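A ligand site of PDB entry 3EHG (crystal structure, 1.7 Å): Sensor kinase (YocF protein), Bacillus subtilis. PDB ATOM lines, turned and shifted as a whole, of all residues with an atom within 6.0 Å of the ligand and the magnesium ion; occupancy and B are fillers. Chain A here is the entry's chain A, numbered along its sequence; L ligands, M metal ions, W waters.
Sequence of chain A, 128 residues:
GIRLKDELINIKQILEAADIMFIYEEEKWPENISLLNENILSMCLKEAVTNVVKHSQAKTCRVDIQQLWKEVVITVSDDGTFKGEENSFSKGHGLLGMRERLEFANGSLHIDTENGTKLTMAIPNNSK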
ATOM      1  N   GLU A  47      12.648 -21.275 -28.445  1.00  0.00           N
ATOM      2  CA  GLU A  47      12.822 -22.392 -27.484  1.00  0.00           C
ATOM      3  C   GLU A  47      14.125 -22.284 -26.661  1.00  0.00           C
ATOM      4  O   GLU A  47      14.124 -22.569 -25.443  1.00  0.00           O
ATOM      5  CB  GLU A  47      12.809 -23.728 -28.207  1.00  0.00           C
ATOM      6  CG  GLU A  47      13.201 -24.945 -27.334  1.00  0.00           C
ATOM      7  CD  GLU A  47      12.359 -25.207 -26.082  1.00  0.00           C
ATOM      8  OE1 GLU A  47      11.257 -24.608 -25.842  1.00  0.00           O
ATOM      9  OE2 GLU A  47      12.790 -26.087 -25.328  1.00  0.00           O
ATOM     10  N   ALA A  48      15.218 -21.884 -27.297  1.00  0.00           N
ATOM     11  CA  ALA A  48      16.530 -21.720 -26.584  1.00  0.00           C
ATOM     12  C   ALA A  48      16.309 -20.728 -25.442  1.00  0.00           C
ATOM     13  O   ALA A  48      16.706 -20.974 -24.331  1.00  0.00           O
ATOM     14  CB  ALA A  48      17.567 -21.239 -27.536  1.00  0.00           C
ATOM     15  N   THR A  50      13.266 -19.717 -24.067  1.00  0.00           N
ATOM     16  CA  THR A  50      12.306 -20.340 -23.115  1.00  0.00           C
ATOM     17  C   THR A  50      13.102 -21.168 -22.115  1.00  0.00           C
ATOM     18  O   THR A  50      12.845 -21.153 -20.915  1.00  0.00           O
ATOM     19  CB  THR A  50      11.305 -21.229 -23.842  1.00  0.00           C
ATOM     20  OG1 THR A  50      10.552 -20.387 -24.736  1.00  0.00           O
ATOM     21  CG2 THR A  50      10.371 -21.926 -22.873  1.00  0.00           C
ATOM     22  N   ASN A  51      14.098 -21.929 -22.617  1.00  0.00           N
ATOM     23  CA  ASN A  51      14.845 -22.801 -21.737  1.00  0.00           C
ATOM     24  C   ASN A  51      15.715 -21.981 -20.745  1.00  0.00           C
ATOM     25  O   ASN A  51      15.888 -22.361 -19.601  1.00  0.00           O
ATOM     26  CB  ASN A  51      15.761 -23.745 -22.518  1.00  0.00           C
ATOM     27  CG  ASN A  51      15.039 -24.943 -23.101  1.00  0.00           C
ATOM     28  OD1 ASN A  51      13.924 -25.288 -22.709  1.00  0.00           O
ATOM     29  ND2 ASN A  51      15.705 -25.588 -24.085  1.00  0.00           N
ATOM     30  N   VAL A  52      16.301 -20.900 -21.243  1.00  0.00           N
ATOM     31  CA  VAL A  52      17.090 -20.014 -20.383  1.00  0.00           C
ATOM     32  C   VAL A  52      16.157 -19.533 -19.248  1.00  0.00           C
ATOM     33  O   VAL A  52      16.514 -19.605 -18.069  1.00  0.00           O
ATOM     34  CB  VAL A  52      17.660 -18.802 -21.150  1.00  0.00           C
ATOM     35  CG1 VAL A  52      18.241 -17.743 -20.191  1.00  0.00           C
ATOM     36  CG2 VAL A  52      18.729 -19.301 -22.162  1.00  0.00           C
ATOM     37  N   LYS A  54      13.235 -20.658 -18.036  1.00  0.00           N
ATOM     38  CA  LYS A  54      12.555 -21.684 -17.220  1.00  0.00           C
ATOM     39  C   LYS A  54      13.524 -22.420 -16.358  1.00  0.00           C
ATOM     40  O   LYS A  54      13.133 -22.917 -15.299  1.00  0.00           O
ATOM     41  CB  LYS A  54      11.940 -22.784 -18.124  1.00  0.00           C
ATOM     42  CG  LYS A  54      10.759 -22.386 -18.929  1.00  0.00           C
ATOM     43  CD  LYS A  54       9.863 -23.589 -19.288  1.00  0.00           C
ATOM     44  CE  LYS A  54      10.507 -24.793 -19.948  1.00  0.00           C
ATOM     45  NZ  LYS A  54       9.308 -25.656 -20.385  1.00  0.00           N
ATOM     46  N   HIS A  55      14.789 -22.579 -16.820  1.00  0.00           N
ATOM     47  CA  HIS A  55      15.713 -23.487 -16.146  1.00  0.00           C
ATOM     48  C   HIS A  55      17.040 -22.900 -15.598  1.00  0.00           C
ATOM     49  O   HIS A  55      17.575 -23.425 -14.653  1.00  0.00           O
ATOM     50  CB  HIS A  55      16.155 -24.656 -17.062  1.00  0.00           C
ATOM     51  CG  HIS A  55      15.037 -25.349 -17.772  1.00  0.00           C
ATOM     52  ND1 HIS A  55      14.086 -26.118 -17.116  1.00  0.00           N
ATOM     53  CD2 HIS A  55      14.803 -25.507 -19.116  1.00  0.00           C
ATOM     54  CE1 HIS A  55      13.284 -26.667 -18.017  1.00  0.00           C
ATOM     55  NE2 HIS A  55      13.680 -26.291 -19.231  1.00  0.00           N
ATOM     56  N   SER A  56      17.580 -21.872 -16.221  1.00  0.00           N
ATOM     57  CA  SER A  56      19.018 -21.586 -16.057  1.00  0.00           C
ATOM     58  C   SER A  56      19.389 -20.937 -14.721  1.00  0.00           C
ATOM     59  O   SER A  56      20.458 -21.177 -14.181  1.00  0.00           O
ATOM     60  CB  SER A  56      19.538 -20.705 -17.203  1.00  0.00           C
ATOM     61  OG  SER A  56      19.032 -19.391 -17.154  1.00  0.00           O
ATOM     62  N   GLN A  57      18.485 -20.114 -14.202  1.00  0.00           N
ATOM     63  CA  GLN A  57      18.784 -19.091 -13.154  1.00  0.00           C
ATOM     64  C   GLN A  57      19.896 -18.091 -13.565  1.00  0.00           C
ATOM     65  O   GLN A  57      20.636 -17.547 -12.724  1.00  0.00           O
ATOM     66  CB  GLN A  57      19.062 -19.756 -11.801  1.00  0.00           C
ATOM     67  CG  GLN A  57      17.962 -20.671 -11.330  1.00  0.00           C
ATOM     68  CD  GLN A  57      18.404 -21.621 -10.318  1.00  0.00           C
ATOM     69  OE1 GLN A  57      19.388 -22.345 -10.552  1.00  0.00           O
ATOM     70  NE2 GLN A  57      17.748 -21.642  -9.140  1.00  0.00           N
ATOM     71  N   ASP A  78      23.999 -18.680 -21.830  1.00  0.00           N
ATOM     72  CA  ASP A  78      23.647 -18.065 -20.595  1.00  0.00           C
ATOM     73  C   ASP A  78      24.625 -18.480 -19.497  1.00  0.00           C
ATOM     74  O   ASP A  78      25.353 -19.467 -19.651  1.00  0.00           O
ATOM     75  CB  ASP A  78      22.205 -18.421 -20.252  1.00  0.00           C
ATOM     76  CG  ASP A  78      22.044 -19.875 -19.726  1.00  0.00           C
ATOM     77  OD1 ASP A  78      22.552 -20.162 -18.645  1.00  0.00           O
ATOM     78  OD2 ASP A  78      21.381 -20.741 -20.418  1.00  0.00           O
ATOM     79  N   THR A  81      23.173 -22.283 -14.545  1.00  0.00           N
ATOM     80  CA  THR A  81      23.691 -23.646 -14.424  1.00  0.00           C
ATOM     81  C   THR A  81      22.755 -24.624 -15.107  1.00  0.00           C
ATOM     82  O   THR A  81      21.522 -24.545 -15.015  1.00  0.00           O
ATOM     83  CB  THR A  81      23.918 -24.092 -12.966  1.00  0.00           C
ATOM     84  OG1 THR A  81      22.708 -23.987 -12.205  1.00  0.00           O
ATOM     85  CG2 THR A  81      24.981 -23.224 -12.227  1.00  0.00           C
ATOM     86  N   PHE A  82      23.358 -25.542 -15.866  1.00  0.00           N
ATOM     87  CA  PHE A  82      22.594 -26.522 -16.607  1.00  0.00           C
ATOM     88  C   PHE A  82      21.952 -27.518 -15.658  1.00  0.00           C
ATOM     89  O   PHE A  82      22.576 -28.020 -14.716  1.00  0.00           O
ATOM     90  CB  PHE A  82      23.471 -27.224 -17.670  1.00  0.00           C
ATOM     91  CG  PHE A  82      22.689 -28.094 -18.595  1.00  0.00           C
ATOM     92  CD1 PHE A  82      21.912 -27.541 -19.579  1.00  0.00           C
ATOM     93  CD2 PHE A  82      22.720 -29.511 -18.437  1.00  0.00           C
ATOM     94  CE1 PHE A  82      21.154 -28.338 -20.440  1.00  0.00           C
ATOM     95  CE2 PHE A  82      21.963 -30.323 -19.298  1.00  0.00           C
ATOM     96  CZ  PHE A  82      21.178 -29.713 -20.272  1.00  0.00           C
ATOM     97  N   LYS A  83      20.680 -27.815 -15.903  1.00  0.00           N
ATOM     98  CA  LYS A  83      19.896 -28.627 -14.961  1.00  0.00           C
ATOM     99  C   LYS A  83      19.574 -30.039 -15.460  1.00  0.00           C
ATOM    100  O   LYS A  83      18.938 -30.812 -14.727  1.00  0.00           O
ATOM    101  CB  LYS A  83      18.567 -27.917 -14.649  1.00  0.00           C
ATOM    102  CG  LYS A  83      18.710 -26.520 -14.026  1.00  0.00           C
ATOM    103  CD  LYS A  83      19.593 -26.461 -12.790  1.00  0.00           C
ATOM    104  CE  LYS A  83      19.359 -25.128 -12.041  1.00  0.00           C
ATOM    105  NZ  LYS A  83      19.703 -23.968 -12.968  1.00  0.00           N
ATOM    106  N   GLY A  84      20.008 -30.377 -16.639  1.00  0.00           N
ATOM    107  CA  GLY A  84      19.623 -31.614 -17.268  1.00  0.00           C
ATOM    108  C   GLY A  84      20.530 -32.759 -16.917  1.00  0.00           C
ATOM    109  O   GLY A  84      21.605 -32.588 -16.327  1.00  0.00           O
ATOM    110  N   GLU A  85      20.078 -33.950 -17.258  1.00  0.00           N
ATOM    111  CA  GLU A  85      20.834 -35.182 -16.989  1.00  0.00           C
ATOM    112  C   GLU A  85      21.949 -35.343 -18.025  1.00  0.00           C
ATOM    113  O   GLU A  85      22.054 -34.545 -18.971  1.00  0.00           O
ATOM    114  CB  GLU A  85      19.918 -36.411 -16.975  1.00  0.00           C
ATOM    115  CG  GLU A  85      18.717 -36.280 -16.021  1.00  0.00           C
ATOM    116  CD  GLU A  85      17.785 -37.487 -16.055  1.00  0.00           C
ATOM    117  OE1 GLU A  85      18.058 -38.473 -16.796  1.00  0.00           O
ATOM    118  OE2 GLU A  85      16.758 -37.450 -15.319  1.00  0.00           O
ATOM    119  N   SER A  88      20.369 -35.133 -22.105  1.00  0.00           N
ATOM    120  CA  SER A  88      19.172 -34.290 -21.898  1.00  0.00           C
ATOM    121  C   SER A  88      18.258 -34.186 -23.114  1.00  0.00           C
ATOM    122  O   SER A  88      17.347 -33.412 -23.138  1.00  0.00           O
ATOM    123  CB  SER A  88      19.625 -32.896 -21.514  1.00  0.00           C
ATOM    124  OG  SER A  88      20.169 -32.948 -20.243  1.00  0.00           O
ATOM    125  N   PHE A  89      18.529 -35.003 -24.118  1.00  0.00           N
ATOM    126  CA  PHE A  89      17.763 -35.007 -25.354  1.00  0.00           C
ATOM    127  C   PHE A  89      16.707 -36.100 -25.257  1.00  0.00           C
ATOM    128  O   PHE A  89      17.004 -37.263 -25.529  1.00  0.00           O
ATOM    129  CB  PHE A  89      18.722 -35.285 -26.485  1.00  0.00           C
ATOM    130  CG  PHE A  89      19.619 -34.114 -26.812  1.00  0.00           C
ATOM    131  CD1 PHE A  89      19.243 -33.203 -27.761  1.00  0.00           C
ATOM    132  CD2 PHE A  89      20.811 -33.891 -26.094  1.00  0.00           C
ATOM    133  CE1 PHE A  89      20.004 -32.102 -28.075  1.00  0.00           C
ATOM    134  CE2 PHE A  89      21.592 -32.795 -26.398  1.00  0.00           C
ATOM    135  CZ  PHE A  89      21.203 -31.882 -27.398  1.00  0.00           C
ATOM    136  N   SER A  90      15.496 -35.740 -24.845  1.00  0.00           N
ATOM    137  CA  SER A  90      14.433 -36.744 -24.698  1.00  0.00           C
ATOM    138  C   SER A  90      13.285 -36.462 -25.641  1.00  0.00           C
ATOM    139  O   SER A  90      12.957 -35.294 -25.933  1.00  0.00           O
ATOM    140  CB  SER A  90      13.936 -36.811 -23.249  1.00  0.00           C
ATOM    141  OG  SER A  90      13.488 -35.532 -22.873  1.00  0.00           O
ATOM    142  N   GLY A  92       9.777 -35.768 -26.982  1.00  0.00           N
ATOM    143  CA  GLY A  92       8.686 -34.926 -26.586  1.00  0.00           C
ATOM    144  C   GLY A  92       9.081 -33.581 -26.049  1.00  0.00           C
ATOM    145  O   GLY A  92       8.215 -32.832 -25.591  1.00  0.00           O
ATOM    146  N   HIS A  93      10.383 -33.251 -26.103  1.00  0.00           N
ATOM    147  CA  HIS A  93      10.889 -32.014 -25.470  1.00  0.00           C
ATOM    148  C   HIS A  93      11.754 -31.254 -26.439  1.00  0.00           C
ATOM    149  O   HIS A  93      12.076 -31.781 -27.535  1.00  0.00           O
ATOM    150  CB  HIS A  93      11.565 -32.325 -24.124  1.00  0.00           C
ATOM    151  CG  HIS A  93      10.628 -32.928 -23.141  1.00  0.00           C
ATOM    152  ND1 HIS A  93       9.619 -32.207 -22.516  1.00  0.00           N
ATOM    153  CD2 HIS A  93      10.533 -34.180 -22.664  1.00  0.00           C
ATOM    154  CE1 HIS A  93       8.936 -33.006 -21.717  1.00  0.00           C
ATOM    155  NE2 HIS A  93       9.472 -34.212 -21.777  1.00  0.00           N
ATOM    156  N   GLY A  94      12.102 -29.999 -26.061  1.00  0.00           N
ATOM    157  CA  GLY A  94      12.624 -29.017 -26.948  1.00  0.00           C
ATOM    158  C   GLY A  94      14.030 -29.273 -27.460  1.00  0.00           C
ATOM    159  O   GLY A  94      14.311 -28.998 -28.635  1.00  0.00           O
ATOM    160  N   LEU A  95      14.927 -29.811 -26.617  1.00  0.00           N
ATOM    161  CA  LEU A  95      16.329 -30.025 -27.132  1.00  0.00           C
ATOM    162  C   LEU A  95      16.351 -31.032 -28.297  1.00  0.00           C
ATOM    163  O   LEU A  95      16.906 -30.718 -29.360  1.00  0.00           O
ATOM    164  CB  LEU A  95      17.328 -30.418 -26.054  1.00  0.00           C
ATOM    165  CG  LEU A  95      17.698 -29.282 -25.104  1.00  0.00           C
ATOM    166  CD1 LEU A  95      18.520 -29.896 -23.894  1.00  0.00           C
ATOM    167  CD2 LEU A  95      18.470 -28.175 -25.848  1.00  0.00           C
ATOM    168  N   LEU A  96      15.710 -32.158 -28.091  1.00  0.00           N
ATOM    169  CA  LEU A  96      15.665 -33.182 -29.128  1.00  0.00           C
ATOM    170  C   LEU A  96      14.771 -32.701 -30.297  1.00  0.00           C
ATOM    171  O   LEU A  96      15.055 -33.002 -31.451  1.00  0.00           O
ATOM    172  CB  LEU A  96      15.222 -34.481 -28.600  1.00  0.00           C
ATOM    173  CG  LEU A  96      15.267 -35.635 -29.600  1.00  0.00           C
ATOM    174  CD1 LEU A  96      16.680 -35.767 -30.256  1.00  0.00           C
ATOM    175  CD2 LEU A  96      14.786 -36.900 -28.979  1.00  0.00           C
ATOM    176  N   MET A  98      14.321 -29.544 -31.355  1.00  0.00           N
ATOM    177  CA  MET A  98      15.070 -28.615 -32.147  1.00  0.00           C
ATOM    178  C   MET A  98      16.123 -29.378 -32.977  1.00  0.00           C
ATOM    179  O   MET A  98      16.272 -29.110 -34.150  1.00  0.00           O
ATOM    180  CB  MET A  98      15.736 -27.569 -31.274  1.00  0.00           C
ATOM    181  CG  MET A  98      14.820 -26.497 -30.660  1.00  0.00           C
ATOM    182  SD  MET A  98      15.801 -25.275 -29.781  1.00  0.00           S
ATOM    183  CE  MET A  98      16.499 -26.238 -28.413  1.00  0.00           C
ATOM    184  N   ILE A 111      25.448 -28.499 -28.119  1.00  0.00           N
ATOM    185  CA  ILE A 111      25.283 -27.969 -26.777  1.00  0.00           C
ATOM    186  C   ILE A 111      26.570 -28.102 -26.003  1.00  0.00           C
ATOM    187  O   ILE A 111      27.260 -29.136 -26.002  1.00  0.00           O
ATOM    188  CB  ILE A 111      24.025 -28.635 -26.046  1.00  0.00           C
ATOM    189  CG1 ILE A 111      23.707 -27.888 -24.736  1.00  0.00           C
ATOM    190  CG2 ILE A 111      24.240 -30.069 -25.816  1.00  0.00           C
ATOM    191  CD1 ILE A 111      22.320 -28.244 -24.141  1.00  0.00           C
ATOM    192  N   THR A 117      25.100 -22.699 -20.072  1.00  0.00           N
ATOM    193  CA  THR A 117      24.592 -23.513 -21.174  1.00  0.00           C
ATOM    194  C   THR A 117      24.749 -22.694 -22.428  1.00  0.00           C
ATOM    195  O   THR A 117      24.297 -21.547 -22.480  1.00  0.00           O
ATOM    196  CB  THR A 117      23.110 -23.845 -20.997  1.00  0.00           C
ATOM    197  OG1 THR A 117      22.964 -24.473 -19.697  1.00  0.00           O
ATOM    198  CG2 THR A 117      22.546 -24.713 -22.161  1.00  0.00           C
HETATM  199  P1  LIG L   1       9.964 -28.552 -23.072  1.00  0.00           P
HETATM  200  O1  LIG L   1       9.227 -29.780 -23.591  1.00  0.00           O
HETATM  201  O2  LIG L   1       9.075 -27.400 -22.639  1.00  0.00           O
HETATM  202  O3  LIG L   1      11.111 -28.119 -23.968  1.00  0.00           O
HETATM  203  P2  LIG L   1      12.055 -28.852 -21.181  1.00  0.00           P
HETATM  204  O4  LIG L   1      12.134 -29.348 -19.785  1.00  0.00           O
HETATM  205  O5  LIG L   1      12.314 -27.389 -21.484  1.00  0.00           O
HETATM  206  O6  LIG L   1      10.615 -29.172 -21.730  1.00  0.00           O
HETATM  207  P3  LIG L   1      14.222 -29.459 -23.014  1.00  0.00           P
HETATM  208  O7  LIG L   1      14.050 -28.117 -23.611  1.00  0.00           O
HETATM  209  O8  LIG L   1      14.451 -30.623 -23.934  1.00  0.00           O
HETATM  210  O9  LIG L   1      12.914 -29.836 -22.104  1.00  0.00           O
HETATM  211  O10 LIG L   1      15.416 -29.379 -21.983  1.00  0.00           O
HETATM  212  C1  LIG L   1      15.725 -30.587 -21.239  1.00  0.00           C
HETATM  213  C2  LIG L   1      16.347 -30.241 -19.913  1.00  0.00           C
HETATM  214  O11 LIG L   1      17.612 -29.599 -20.110  1.00  0.00           O
HETATM  215  C3  LIG L   1      15.530 -29.260 -19.070  1.00  0.00           C
HETATM  216  O12 LIG L   1      14.381 -29.815 -18.345  1.00  0.00           O
HETATM  217  C4  LIG L   1      16.609 -28.752 -18.152  1.00  0.00           C
HETATM  218  O13 LIG L   1      16.897 -29.669 -17.081  1.00  0.00           O
HETATM  219  C5  LIG L   1      17.796 -28.645 -19.061  1.00  0.00           C
HETATM  220  N1  LIG L   1      18.024 -27.331 -19.731  1.00  0.00           N
HETATM  221  C6  LIG L   1      17.759 -27.044 -21.011  1.00  0.00           C
HETATM  222  N2  LIG L   1      18.145 -25.782 -21.323  1.00  0.00           N
HETATM  223  C7  LIG L   1      18.717 -25.321 -20.165  1.00  0.00           C
HETATM  224  C8  LIG L   1      19.333 -24.063 -19.745  1.00  0.00           C
HETATM  225  N3  LIG L   1      19.455 -23.071 -20.616  1.00  0.00           N
HETATM  226  N4  LIG L   1      19.757 -23.910 -18.515  1.00  0.00           N
HETATM  227  C9  LIG L   1      19.618 -24.913 -17.589  1.00  0.00           C
HETATM  228  N5  LIG L   1      19.031 -26.116 -17.828  1.00  0.00           N
HETATM  229  C10 LIG L   1      18.580 -26.326 -19.109  1.00  0.00           C
HETATM  230 MG    MG M   1      12.566 -26.726 -23.408  1.00  0.00          MG
HETATM  231  O   HOH W   1      15.251 -33.936 -21.585  1.00  0.00           O
HETATM  232  O   HOH W   2      11.014 -25.343 -23.216  1.00  0.00           O
HETATM  233  O   HOH W   3      14.798 -32.328 -17.159  1.00  0.00           O
HETATM  234  O   HOH W   4      19.104 -22.425 -23.636  1.00  0.00           O
HETATM  235  O   HOH W   5      14.724 -32.905 -25.455  1.00  0.00           O
HETATM  236  O   HOH W   6      22.399 -22.792 -17.783  1.00  0.00           O
HETATM  237  O   HOH W   7      14.920 -29.135 -15.170  1.00  0.00           O
HETATM  238  O   HOH W   8      18.443 -25.102 -24.074  1.00  0.00           O
HETATM  239  O   HOH W   9      11.377 -32.154 -19.310  1.00  0.00           O
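Water W2 lies within hydrogen-bond range of OE1 of Glu 47 (2.7 Å), O2 of the ligand (2.9 Å) and NZ of Lys 54 (3.3 Å).
Water W8 lies within hydrogen-bond range of ND2 of Asn 51 (2.8 Å) and N2 of the ligand (2.8 Å).
Water W6 lies within hydrogen-bond range of OG1 of Thr 117 (2.6 Å), OD1 of Asp 78 (2.8 Å), N4 of the ligand (3.0 Å), N of Thr 81 (3.4 Å) and N of Phe 82 (3.5 Å).
Water W4 bridges the backbone carbonyl oxygen of Ala 48 and a nitrogen (N3) of the ligand.
Water W1 lies within hydrogen-bond range of the backbone carbonyl oxygen of Ser 88 (2.7 Å) and the side-chain hydroxyl of Ser 90 (2.7 Å).
N5 of the ligand is in hydrogen-bond range of N of Lys 83, 3.1 Å away.
NZ of Lys 54 lies within salt-bridge range of O2 of the ligand, at 2.9 Å.
O8 of the ligand is in hydrogen-bond range of N of Gly 94 (3.2 Å).
NE2 of His 55 sits close to O4 of the ligand (3.5 Å).
An oxygen (O13) of the ligand lies close to the backbone carbonyl oxygen of Lys 83.
A nitrogen (N3) of the ligand is in hydrogen-bond range of the side-chain carboxylate (OD2) of Asp 78, at 3.0 Å.
The backbone NH (N) of Leu 95 is in hydrogen-bond range of an oxygen (O8) of the ligand, at 2.8 Å.
OG1 of Thr 117 lies within hydrogen-bond range of N4 of the ligand (3.5 Å).
O1 of the ligand lies within hydrogen-bond range of ND1 of His 93 (2.7 Å).
The backbone NH (N) of Gly 84 lies within hydrogen-bond range of an oxygen (O13) of the ligand, 3.2 Å away.
CA of Val 52 touches N3 of the ligand (3.9 Å).
Ser 56 touches the ligand.
Thr 81 touches the ligand.
Phe 82 touches the ligand.
Ser 88 touches the ligand.
O of Gly 92 touches O1 of the ligand (3.8 Å).
Of the 26 residues printed, 17 come within 4 Å of the ligand.
The nearest printed residue that does not touch the ligand is Leu 96 (4.6 Å).
OE2 of Glu 47 is bound to the magnesium ion (2.0 Å).
The magnesium ion is bound by O7 of the ligand, 2.0 Å away.
The magnesium ion is bound by O5 of the ligand (2.1 Å).
Water W2 is bound to the magnesium ion, 2.1 Å away.
O3 of the ligand binds the magnesium ion (2.1 Å).
OD1 of Asn 51 is bound to the magnesium ion (2.1 Å).
Within 4 Å of the magnesium ion: Glu 47 and Asn 51.
The nearest printed residue that does not touch the magnesium ion is Gly 94 (4.2 Å).
The side-chain hydroxyl (OG) of Ser 88 is in hydrogen-bond range of the backbone carbonyl oxygen (O) of Glu 85, 2.8 Å away.
The backbone NH (N) of Asp 78 sits at hydrogen-bond distance from the backbone carbonyl oxygen (O) of Thr 117, at 3.0 Å.
N of Thr 81 sits at hydrogen-bond distance from O of Ser 56, 3.0 Å away.
O of His 55 lies within hydrogen-bond range of NZ of Lys 83.
The backbone carbonyl oxygen of Thr 81 lies within hydrogen-bond range of the side-chain amino group of Lys 83, at 2.8 Å.
The side-chain hydroxyl (OG) of Ser 56 lies within hydrogen-bond range of the backbone carbonyl oxygen (O) of Val 52 (2.7 Å).
NZ of Lys 83 lies within hydrogen-bond range of OE1 of Gln 57, 2.9 Å away.
The side-chain amino group of Lys 83 sits at hydrogen-bond distance from the backbone carbonyl oxygen of Ser 56 (3.1 Å).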
